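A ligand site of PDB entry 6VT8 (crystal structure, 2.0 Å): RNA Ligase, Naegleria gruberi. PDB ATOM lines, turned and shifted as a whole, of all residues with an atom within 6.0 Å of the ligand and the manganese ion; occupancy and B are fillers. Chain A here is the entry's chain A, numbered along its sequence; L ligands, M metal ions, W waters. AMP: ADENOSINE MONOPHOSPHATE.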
ATOM      1  N   THR A 146     -19.869  -0.760  17.683  1.00  0.00           N
ATOM      2  CA  THR A 146     -19.357   0.556  18.023  1.00  0.00           C
ATOM      3  C   THR A 146     -17.834   0.608  18.105  1.00  0.00           C
ATOM      4  O   THR A 146     -17.292   1.565  18.679  1.00  0.00           O
ATOM      5  CB  THR A 146     -19.947   1.051  19.343  1.00  0.00           C
ATOM      6  OG1 THR A 146     -19.441   0.269  20.442  1.00  0.00           O
ATOM      7  CG2 THR A 146     -21.466   0.971  19.296  1.00  0.00           C
ATOM      8  N   ASP A 147     -17.128  -0.380  17.567  1.00  0.00           N
ATOM      9  CA  ASP A 147     -15.672  -0.308  17.590  1.00  0.00           C
ATOM     10  C   ASP A 147     -15.182   0.922  16.807  1.00  0.00           C
ATOM     11  O   ASP A 147     -15.815   1.354  15.843  1.00  0.00           O
ATOM     12  CB  ASP A 147     -15.070  -1.593  17.023  1.00  0.00           C
ATOM     13  CG  ASP A 147     -15.471  -2.827  17.839  1.00  0.00           C
ATOM     14  OD1 ASP A 147     -15.145  -2.883  19.044  1.00  0.00           O
ATOM     15  OD2 ASP A 147     -16.142  -3.720  17.275  1.00  0.00           O
ATOM     16  N   GLN A 148     -14.073   1.506  17.267  1.00  0.00           N
ATOM     17  CA  GLN A 148     -13.438   2.625  16.586  1.00  0.00           C
ATOM     18  C   GLN A 148     -11.969   2.300  16.278  1.00  0.00           C
ATOM     19  O   GLN A 148     -11.294   1.658  17.083  1.00  0.00           O
ATOM     20  CB  GLN A 148     -13.494   3.899  17.430  1.00  0.00           C
ATOM     21  CG  GLN A 148     -14.923   4.361  17.768  1.00  0.00           C
ATOM     22  CD  GLN A 148     -15.591   5.050  16.596  1.00  0.00           C
ATOM     23  OE1 GLN A 148     -14.947   5.355  15.578  1.00  0.00           O
ATOM     24  NE2 GLN A 148     -16.894   5.310  16.725  1.00  0.00           N
ATOM     25  N   ARG A 150      -7.969   3.229  15.770  1.00  0.00           N
ATOM     26  CA  ARG A 150      -7.035   4.116  16.447  1.00  0.00           C
ATOM     27  C   ARG A 150      -6.363   5.068  15.474  1.00  0.00           C
ATOM     28  O   ARG A 150      -5.973   4.678  14.365  1.00  0.00           O
ATOM     29  CB  ARG A 150      -5.951   3.327  17.188  1.00  0.00           C
ATOM     30  CG  ARG A 150      -6.433   2.410  18.312  1.00  0.00           C
ATOM     31  CD  ARG A 150      -5.238   1.777  19.026  1.00  0.00           C
ATOM     32  NE  ARG A 150      -5.553   1.242  20.354  1.00  0.00           N
ATOM     33  CZ  ARG A 150      -5.947  -0.013  20.564  1.00  0.00           C
ATOM     34  NH1 ARG A 150      -6.102  -0.846  19.523  1.00  0.00           N
ATOM     35  NH2 ARG A 150      -6.195  -0.416  21.802  1.00  0.00           N
ATOM     36  N   THR A 169     -15.596  14.174  21.195  1.00  0.00           N
ATOM     37  CA  THR A 169     -16.270  13.789  22.432  1.00  0.00           C
ATOM     38  C   THR A 169     -15.301  13.086  23.370  1.00  0.00           C
ATOM     39  O   THR A 169     -14.295  12.516  22.935  1.00  0.00           O
ATOM     40  CB  THR A 169     -17.455  12.875  22.165  1.00  0.00           C
ATOM     41  OG1 THR A 169     -17.028  11.728  21.405  1.00  0.00           O
ATOM     42  CG2 THR A 169     -18.568  13.607  21.415  1.00  0.00           C
ATOM     43  N   VAL A 170     -15.603  13.138  24.654  1.00  0.00           N
ATOM     44  CA  VAL A 170     -14.798  12.402  25.624  1.00  0.00           C
ATOM     45  C   VAL A 170     -15.113  10.919  25.496  1.00  0.00           C
ATOM     46  O   VAL A 170     -16.279  10.520  25.328  1.00  0.00           O
ATOM     47  CB  VAL A 170     -15.045  12.923  27.044  1.00  0.00           C
ATOM     48  CG1 VAL A 170     -14.288  12.063  28.044  1.00  0.00           C
ATOM     49  CG2 VAL A 170     -14.619  14.403  27.157  1.00  0.00           C
ATOM     50  N   LYS A 171     -14.068  10.100  25.510  1.00  0.00           N
ATOM     51  CA  LYS A 171     -14.178   8.643  25.482  1.00  0.00           C
ATOM     52  C   LYS A 171     -14.393   8.169  26.922  1.00  0.00           C
ATOM     53  O   LYS A 171     -13.493   8.241  27.754  1.00  0.00           O
ATOM     54  CB  LYS A 171     -12.942   8.024  24.845  1.00  0.00           C
ATOM     55  CG  LYS A 171     -13.069   6.537  24.511  1.00  0.00           C
ATOM     56  CD  LYS A 171     -11.778   5.939  23.956  1.00  0.00           C
ATOM     57  CE  LYS A 171     -12.062   4.649  23.171  1.00  0.00           C
ATOM     58  NZ  LYS A 171     -12.353   3.472  24.077  1.00  0.00           N
ATOM     59  N   LEU A 172     -15.623   7.752  27.228  1.00  0.00           N
ATOM     60  CA  LEU A 172     -15.940   7.239  28.552  1.00  0.00           C
ATOM     61  C   LEU A 172     -15.550   5.761  28.639  1.00  0.00           C
ATOM     62  O   LEU A 172     -15.714   5.001  27.678  1.00  0.00           O
ATOM     63  CB  LEU A 172     -17.426   7.406  28.846  1.00  0.00           C
ATOM     64  CG  LEU A 172     -17.906   8.851  28.864  1.00  0.00           C
ATOM     65  CD1 LEU A 172     -19.423   8.953  29.195  1.00  0.00           C
ATOM     66  CD2 LEU A 172     -17.064   9.673  29.838  1.00  0.00           C
ATOM     67  N   ASP A 173     -15.020   5.367  29.805  1.00  0.00           N
ATOM     68  CA  ASP A 173     -14.550   4.010  30.057  1.00  0.00           C
ATOM     69  C   ASP A 173     -15.660   3.239  30.791  1.00  0.00           C
ATOM     70  O   ASP A 173     -15.664   3.140  32.014  1.00  0.00           O
ATOM     71  CB  ASP A 173     -13.269   4.023  30.861  1.00  0.00           C
ATOM     72  CG  ASP A 173     -12.592   2.662  30.916  1.00  0.00           C
ATOM     73  OD1 ASP A 173     -13.221   1.657  30.546  1.00  0.00           O
ATOM     74  OD2 ASP A 173     -11.437   2.604  31.333  1.00  0.00           O
ATOM     75  N   GLY A 174     -16.566   2.665  30.011  1.00  0.00           N
ATOM     76  CA  GLY A 174     -17.598   1.833  30.573  1.00  0.00           C
ATOM     77  C   GLY A 174     -17.752   0.600  29.722  1.00  0.00           C
ATOM     78  O   GLY A 174     -16.775  -0.110  29.483  1.00  0.00           O
ATOM     79  N   SER A 175     -18.956   0.382  29.235  1.00  0.00           N
ATOM     80  CA  SER A 175     -19.229  -0.738  28.341  1.00  0.00           C
ATOM     81  C   SER A 175     -20.198  -0.246  27.282  1.00  0.00           C
ATOM     82  O   SER A 175     -21.075   0.577  27.559  1.00  0.00           O
ATOM     83  CB  SER A 175     -19.788  -1.949  29.123  1.00  0.00           C
ATOM     84  OG  SER A 175     -20.018  -3.060  28.284  1.00  0.00           O
ATOM     85  N   SER A 176     -20.015  -0.730  26.058  1.00  0.00           N
ATOM     86  CA  SER A 176     -20.904  -0.367  24.958  1.00  0.00           C
ATOM     87  C   SER A 176     -22.304  -0.931  25.176  1.00  0.00           C
ATOM     88  O   SER A 176     -22.472  -2.078  25.618  1.00  0.00           O
ATOM     89  CB  SER A 176     -20.330  -0.868  23.641  1.00  0.00           C
ATOM     90  OG  SER A 176     -21.133  -0.518  22.539  1.00  0.00           O
ATOM     91  N   MET A 177     -23.317  -0.130  24.837  1.00  0.00           N
ATOM     92  CA  MET A 177     -24.706  -0.486  25.072  1.00  0.00           C
ATOM     93  C   MET A 177     -25.565   0.085  23.957  1.00  0.00           C
ATOM     94  O   MET A 177     -25.454   1.263  23.624  1.00  0.00           O
ATOM     95  CB  MET A 177     -25.145   0.029  26.456  1.00  0.00           C
ATOM     96  CG  MET A 177     -26.603   0.214  26.651  1.00  0.00           C
ATOM     97  SD  MET A 177     -27.057   0.596  28.371  1.00  0.00           S
ATOM     98  CE  MET A 177     -28.785   0.942  28.061  1.00  0.00           C
ATOM     99  N   ARG A 191     -22.296  -5.229  24.270  1.00  0.00           N
ATOM    100  CA  ARG A 191     -21.318  -5.015  23.208  1.00  0.00           C
ATOM    101  C   ARG A 191     -21.460  -6.032  22.080  1.00  0.00           C
ATOM    102  O   ARG A 191     -21.272  -5.689  20.915  1.00  0.00           O
ATOM    103  CB  ARG A 191     -19.909  -5.067  23.796  1.00  0.00           C
ATOM    104  CG  ARG A 191     -18.797  -4.901  22.755  1.00  0.00           C
ATOM    105  CD  ARG A 191     -17.472  -5.106  23.429  1.00  0.00           C
ATOM    106  NE  ARG A 191     -16.380  -4.781  22.531  1.00  0.00           N
ATOM    107  CZ  ARG A 191     -15.100  -5.011  22.813  1.00  0.00           C
ATOM    108  NH1 ARG A 191     -14.752  -5.551  23.970  1.00  0.00           N
ATOM    109  NH2 ARG A 191     -14.171  -4.695  21.924  1.00  0.00           N
ATOM    110  N   GLY A 227     -24.412   4.021  23.075  1.00  0.00           N
ATOM    111  CA  GLY A 227     -23.729   4.798  24.081  1.00  0.00           C
ATOM    112  C   GLY A 227     -22.986   3.917  25.059  1.00  0.00           C
ATOM    113  O   GLY A 227     -22.874   2.695  24.864  1.00  0.00           O
ATOM    114  N   GLU A 228     -22.448   4.540  26.080  1.00  0.00           N
ATOM    115  CA  GLU A 228     -21.634   3.898  27.093  1.00  0.00           C
ATOM    116  C   GLU A 228     -22.413   3.867  28.399  1.00  0.00           C
ATOM    117  O   GLU A 228     -22.856   4.925  28.874  1.00  0.00           O
ATOM    118  CB  GLU A 228     -20.303   4.641  27.275  1.00  0.00           C
ATOM    119  CG  GLU A 228     -19.188   3.864  27.929  1.00  0.00           C
ATOM    120  CD  GLU A 228     -18.457   2.931  26.964  1.00  0.00           C
ATOM    121  OE1 GLU A 228     -18.953   2.740  25.828  1.00  0.00           O
ATOM    122  OE2 GLU A 228     -17.383   2.403  27.350  1.00  0.00           O
ATOM    123  N   PHE A 249     -23.484   8.273  22.410  1.00  0.00           N
ATOM    124  CA  PHE A 249     -22.470   8.818  21.506  1.00  0.00           C
ATOM    125  C   PHE A 249     -22.782   8.621  20.016  1.00  0.00           C
ATOM    126  O   PHE A 249     -22.079   9.206  19.181  1.00  0.00           O
ATOM    127  CB  PHE A 249     -21.062   8.266  21.824  1.00  0.00           C
ATOM    128  CG  PHE A 249     -20.968   6.765  21.919  1.00  0.00           C
ATOM    129  CD1 PHE A 249     -21.184   5.962  20.799  1.00  0.00           C
ATOM    130  CD2 PHE A 249     -20.594   6.152  23.106  1.00  0.00           C
ATOM    131  CE1 PHE A 249     -21.085   4.577  20.891  1.00  0.00           C
ATOM    132  CE2 PHE A 249     -20.486   4.778  23.200  1.00  0.00           C
ATOM    133  CZ  PHE A 249     -20.743   3.975  22.102  1.00  0.00           C
ATOM    134  N   ASP A 250     -23.810   7.850  19.658  1.00  0.00           N
ATOM    135  CA  ASP A 250     -24.122   7.578  18.263  1.00  0.00           C
ATOM    136  C   ASP A 250     -25.572   7.138  18.138  1.00  0.00           C
ATOM    137  O   ASP A 250     -26.120   6.505  19.046  1.00  0.00           O
ATOM    138  CB  ASP A 250     -23.203   6.475  17.686  1.00  0.00           C
ATOM    139  CG  ASP A 250     -22.085   7.014  16.801  1.00  0.00           C
ATOM    140  OD1 ASP A 250     -22.319   7.991  16.043  1.00  0.00           O
ATOM    141  OD2 ASP A 250     -20.970   6.441  16.863  1.00  0.00           O
ATOM    142  N   VAL A 282     -22.460  11.725  25.885  1.00  0.00           N
ATOM    143  CA  VAL A 282     -21.029  11.818  26.200  1.00  0.00           C
ATOM    144  C   VAL A 282     -20.615  13.285  26.079  1.00  0.00           C
ATOM    145  O   VAL A 282     -21.161  13.992  25.220  1.00  0.00           O
ATOM    146  CB  VAL A 282     -20.168  10.920  25.273  1.00  0.00           C
ATOM    147  CG1 VAL A 282     -20.490   9.419  25.502  1.00  0.00           C
ATOM    148  CG2 VAL A 282     -20.333  11.316  23.810  1.00  0.00           C
ATOM    149  N   PRO A 283     -19.679  13.765  26.893  1.00  0.00           N
ATOM    150  CA  PRO A 283     -19.294  15.191  26.812  1.00  0.00           C
ATOM    151  C   PRO A 283     -18.811  15.540  25.425  1.00  0.00           C
ATOM    152  O   PRO A 283     -18.029  14.801  24.819  1.00  0.00           O
ATOM    153  CB  PRO A 283     -18.162  15.322  27.833  1.00  0.00           C
ATOM    154  CG  PRO A 283     -18.359  14.173  28.769  1.00  0.00           C
ATOM    155  CD  PRO A 283     -18.951  13.052  27.951  1.00  0.00           C
ATOM    156  N   VAL A 316     -12.777  10.633  21.043  1.00  0.00           N
ATOM    157  CA  VAL A 316     -13.275  10.033  19.814  1.00  0.00           C
ATOM    158  C   VAL A 316     -13.670  11.168  18.883  1.00  0.00           C
ATOM    159  O   VAL A 316     -14.323  12.130  19.300  1.00  0.00           O
ATOM    160  CB  VAL A 316     -14.483   9.103  20.083  1.00  0.00           C
ATOM    161  CG1 VAL A 316     -15.035   8.535  18.780  1.00  0.00           C
ATOM    162  CG2 VAL A 316     -14.104   7.969  21.028  1.00  0.00           C
ATOM    163  N   LYS A 318     -15.578  12.274  15.332  1.00  0.00           N
ATOM    164  CA  LYS A 318     -16.548  11.873  14.329  1.00  0.00           C
ATOM    165  C   LYS A 318     -16.705  12.985  13.306  1.00  0.00           C
ATOM    166  O   LYS A 318     -17.152  14.094  13.642  1.00  0.00           O
ATOM    167  CB  LYS A 318     -17.886  11.499  14.966  1.00  0.00           C
ATOM    168  CG  LYS A 318     -17.804  10.267  15.890  1.00  0.00           C
ATOM    169  CD  LYS A 318     -19.122  10.075  16.667  1.00  0.00           C
ATOM    170  CE  LYS A 318     -18.974   9.103  17.845  1.00  0.00           C
ATOM    171  NZ  LYS A 318     -18.378   9.749  19.055  1.00  0.00           N
ATOM    172  N   LYS A 327     -10.672   6.853  17.250  1.00  0.00           N
ATOM    173  CA  LYS A 327     -10.421   7.079  18.661  1.00  0.00           C
ATOM    174  C   LYS A 327      -8.973   7.481  18.882  1.00  0.00           C
ATOM    175  O   LYS A 327      -8.069   6.993  18.192  1.00  0.00           O
ATOM    176  CB  LYS A 327     -10.786   5.844  19.513  1.00  0.00           C
ATOM    177  CG  LYS A 327      -9.896   4.579  19.361  1.00  0.00           C
ATOM    178  CD  LYS A 327     -10.410   3.384  20.235  1.00  0.00           C
ATOM    179  CE  LYS A 327      -9.664   2.034  19.950  1.00  0.00           C
ATOM    180  NZ  LYS A 327     -10.491   0.803  20.328  1.00  0.00           N
ATOM    181  N   ILE A 329      -6.744   7.329  22.142  1.00  0.00           N
ATOM    182  CA  ILE A 329      -6.650   6.905  23.525  1.00  0.00           C
ATOM    183  C   ILE A 329      -5.467   7.607  24.183  1.00  0.00           C
ATOM    184  O   ILE A 329      -4.398   7.750  23.574  1.00  0.00           O
ATOM    185  CB  ILE A 329      -6.521   5.372  23.601  1.00  0.00           C
ATOM    186  CG1 ILE A 329      -7.850   4.743  23.185  1.00  0.00           C
ATOM    187  CG2 ILE A 329      -6.098   4.930  25.002  1.00  0.00           C
ATOM    188  CD1 ILE A 329      -7.794   3.243  22.956  1.00  0.00           C
HETATM  189  P   AMP L   1     -12.348   2.019  23.269  1.00  0.00           P
HETATM  190  O1P AMP L   1     -12.926   1.058  24.272  1.00  0.00           O
HETATM  191  O2P AMP L   1     -10.854   1.916  23.070  1.00  0.00           O
HETATM  192  O5' AMP L   1     -13.008   1.653  21.855  1.00  0.00           O
HETATM  193  C5' AMP L   1     -14.206   2.269  21.399  1.00  0.00           C
HETATM  194  C4' AMP L   1     -15.356   2.111  22.374  1.00  0.00           C
HETATM  195  O4' AMP L   1     -15.392   3.226  23.281  1.00  0.00           O
HETATM  196  C3' AMP L   1     -16.749   2.109  21.761  1.00  0.00           C
HETATM  197  O3' AMP L   1     -17.110   0.820  21.292  1.00  0.00           O
HETATM  198  C2' AMP L   1     -17.656   2.604  22.893  1.00  0.00           C
HETATM  199  O2' AMP L   1     -18.143   1.480  23.636  1.00  0.00           O
HETATM  200  C1' AMP L   1     -16.706   3.392  23.796  1.00  0.00           C
HETATM  201  N9  AMP L   1     -16.940   4.862  23.849  1.00  0.00           N
HETATM  202  C8  AMP L   1     -16.804   5.611  24.963  1.00  0.00           C
HETATM  203  N7  AMP L   1     -16.996   6.930  24.713  1.00  0.00           N
HETATM  204  C5  AMP L   1     -17.227   7.052  23.402  1.00  0.00           C
HETATM  205  C6  AMP L   1     -17.509   8.170  22.473  1.00  0.00           C
HETATM  206  N6  AMP L   1     -17.554   9.447  22.878  1.00  0.00           N
HETATM  207  N1  AMP L   1     -17.717   7.877  21.172  1.00  0.00           N
HETATM  208  C2  AMP L   1     -17.649   6.616  20.726  1.00  0.00           C
HETATM  209  N3  AMP L   1     -17.406   5.544  21.508  1.00  0.00           N
HETATM  210  C4  AMP L   1     -17.196   5.693  22.829  1.00  0.00           C
HETATM  211 MN    MN M   1     -13.786   0.861  26.176  1.00  0.00          MN
HETATM  212  O   HOH W   1     -13.372  -1.165  22.803  1.00  0.00           O
HETATM  213  O   HOH W   2     -18.025   4.154  19.124  1.00  0.00           O
HETATM  214  O   HOH W   3     -16.262   0.634  25.799  1.00  0.00           O
HETATM  215  O   HOH W   4     -16.448  -1.408  23.225  1.00  0.00           O
HETATM  216  O   HOH W   5     -14.290   0.716  28.174  1.00  0.00           O
HETATM  217  O   HOH W   6     -13.631   3.214  26.687  1.00  0.00           O
HETATM  218  O   HOH W   7     -13.802  -1.499  25.902  1.00  0.00           O
HETATM  219  O   HOH W   8     -12.718  -0.064  19.452  1.00  0.00           O
HETATM  220  O   HOH W   9     -11.840   0.977  26.935  1.00  0.00           O
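Residues that only touch the manganese ion: Lys 171 (3.6 Å).
The nearest printed residue that does not touch the manganese ion is Glu 228 (4.1 Å).
A phosphorus (P) of the ligand is bonded to the side-chain amino group (NZ) of Lys 171, at 1.7 Å.
O3' of the ligand lies within hydrogen-bond range of O of Thr 146, 2.7 Å away.
O3' of the ligand lies within hydrogen-bond range of OG1 of Thr 146 (2.5 Å).
The side-chain carboxylate (OE1) of Glu 228 sits at hydrogen-bond distance from an oxygen (O2') of the ligand (2.7 Å).
OG1 of Thr 169 sits at hydrogen-bond distance from N6 of the ligand, 2.8 Å away.
A nitrogen (N1) of the ligand sits at hydrogen-bond distance from the side-chain amino group of Lys 318 (2.9 Å).
N6 of the ligand sits at hydrogen-bond distance from O of Val 170 (3.0 Å).
The side-chain amino group of Lys 327 is in salt-bridge range of an oxygen (O2P) of the ligand (3.0 Å).
A nitrogen (N7) of the ligand lies within hydrogen-bond range of the backbone NH (N) of Leu 172.
Water W3 bridges OE2 of Glu 228 and O2' of the ligand.
Water W6 lies within hydrogen-bond range of O of Leu 172 (2.9 Å) and NZ of Lys 171 (2.9 Å).
Water W5 bridges the side-chain carboxylate (OD1) of Asp 173 (2.8 Å) and the backbone carbonyl oxygen (O) of Gly 174 (2.9 Å).
Water W2 lies within hydrogen-bond range of the backbone carbonyl oxygen of Thr 146 (2.7 Å), a nitrogen (N3) of the ligand (2.8 Å) and the side-chain amide nitrogen of Gln 148 (2.9 Å).
Water W8 lies within hydrogen-bond range of the side-chain amino group of Lys 327, an oxygen (O5') of the ligand and the backbone NH of Gln 148.
Water W4 bridges O3' of the ligand and NE of Arg 191.
The manganese ion is bound by water W5 (2.1 Å), water W9 (2.1 Å), O1P of the ligand (2.1 Å), water W7 (2.4 Å), water W6 (2.4 Å) and water W3 (2.5 Å).
The manganese ion has six donor atoms within binding distance.
Merely in contact with the ligand: Ser 176 (3.2 Å), Ile 329 (3.3 Å), Phe 249 (3.4 Å), Val 282 (3.5 Å), Val 316 (3.6 Å) and Asp 147 (3.9 Å).
Hydrophobic or aromatic side chains within 4 Å of the ligand: Phe 249, Val 282, Val 316 and Ile 329.
Within 4 Å of the ligand: Thr 146, Asp 147, Thr 169, Val 170, Lys 171, Leu 172, Ser 176, Glu 228, Phe 249, Val 282, Val 316, Lys 318, Lys 327 and Ile 329.
The nearest printed residue that does not touch the ligand is Gln 148 (4.2 Å).
OG1 of Thr 146 is in hydrogen-bond range of OG of Ser 176 (2.8 Å).
The side-chain carboxylate (OE2) of Glu 228 sits at hydrogen-bond distance from the backbone NH (N) of Ser 175 (3.2 Å).
The side-chain carboxylate (OE2) of Glu 228 sits at hydrogen-bond distance from the backbone NH (N) of Gly 174 (2.8 Å).
The side-chain hydroxyl (OG1) of Thr 169 sits at hydrogen-bond distance from the side-chain amino group (NZ) of Lys 318 (3.4 Å).
The backbone NH (N) of Val 170 lies within hydrogen-bond range of the backbone carbonyl oxygen (O) of Pro 283, at 2.9 Å.
The side-chain amino group (NZ) of Lys 327 lies close to the backbone carbonyl oxygen (O) of Gln 148, at 3.5 Å.
The backbone NH of Arg 191 lies within hydrogen-bond range of the backbone carbonyl oxygen of Ser 176.
The guanidinium group (NH2) of Arg 191 is in salt-bridge range of the side-chain carboxylate (OD1) of Asp 147 (3.5 Å).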
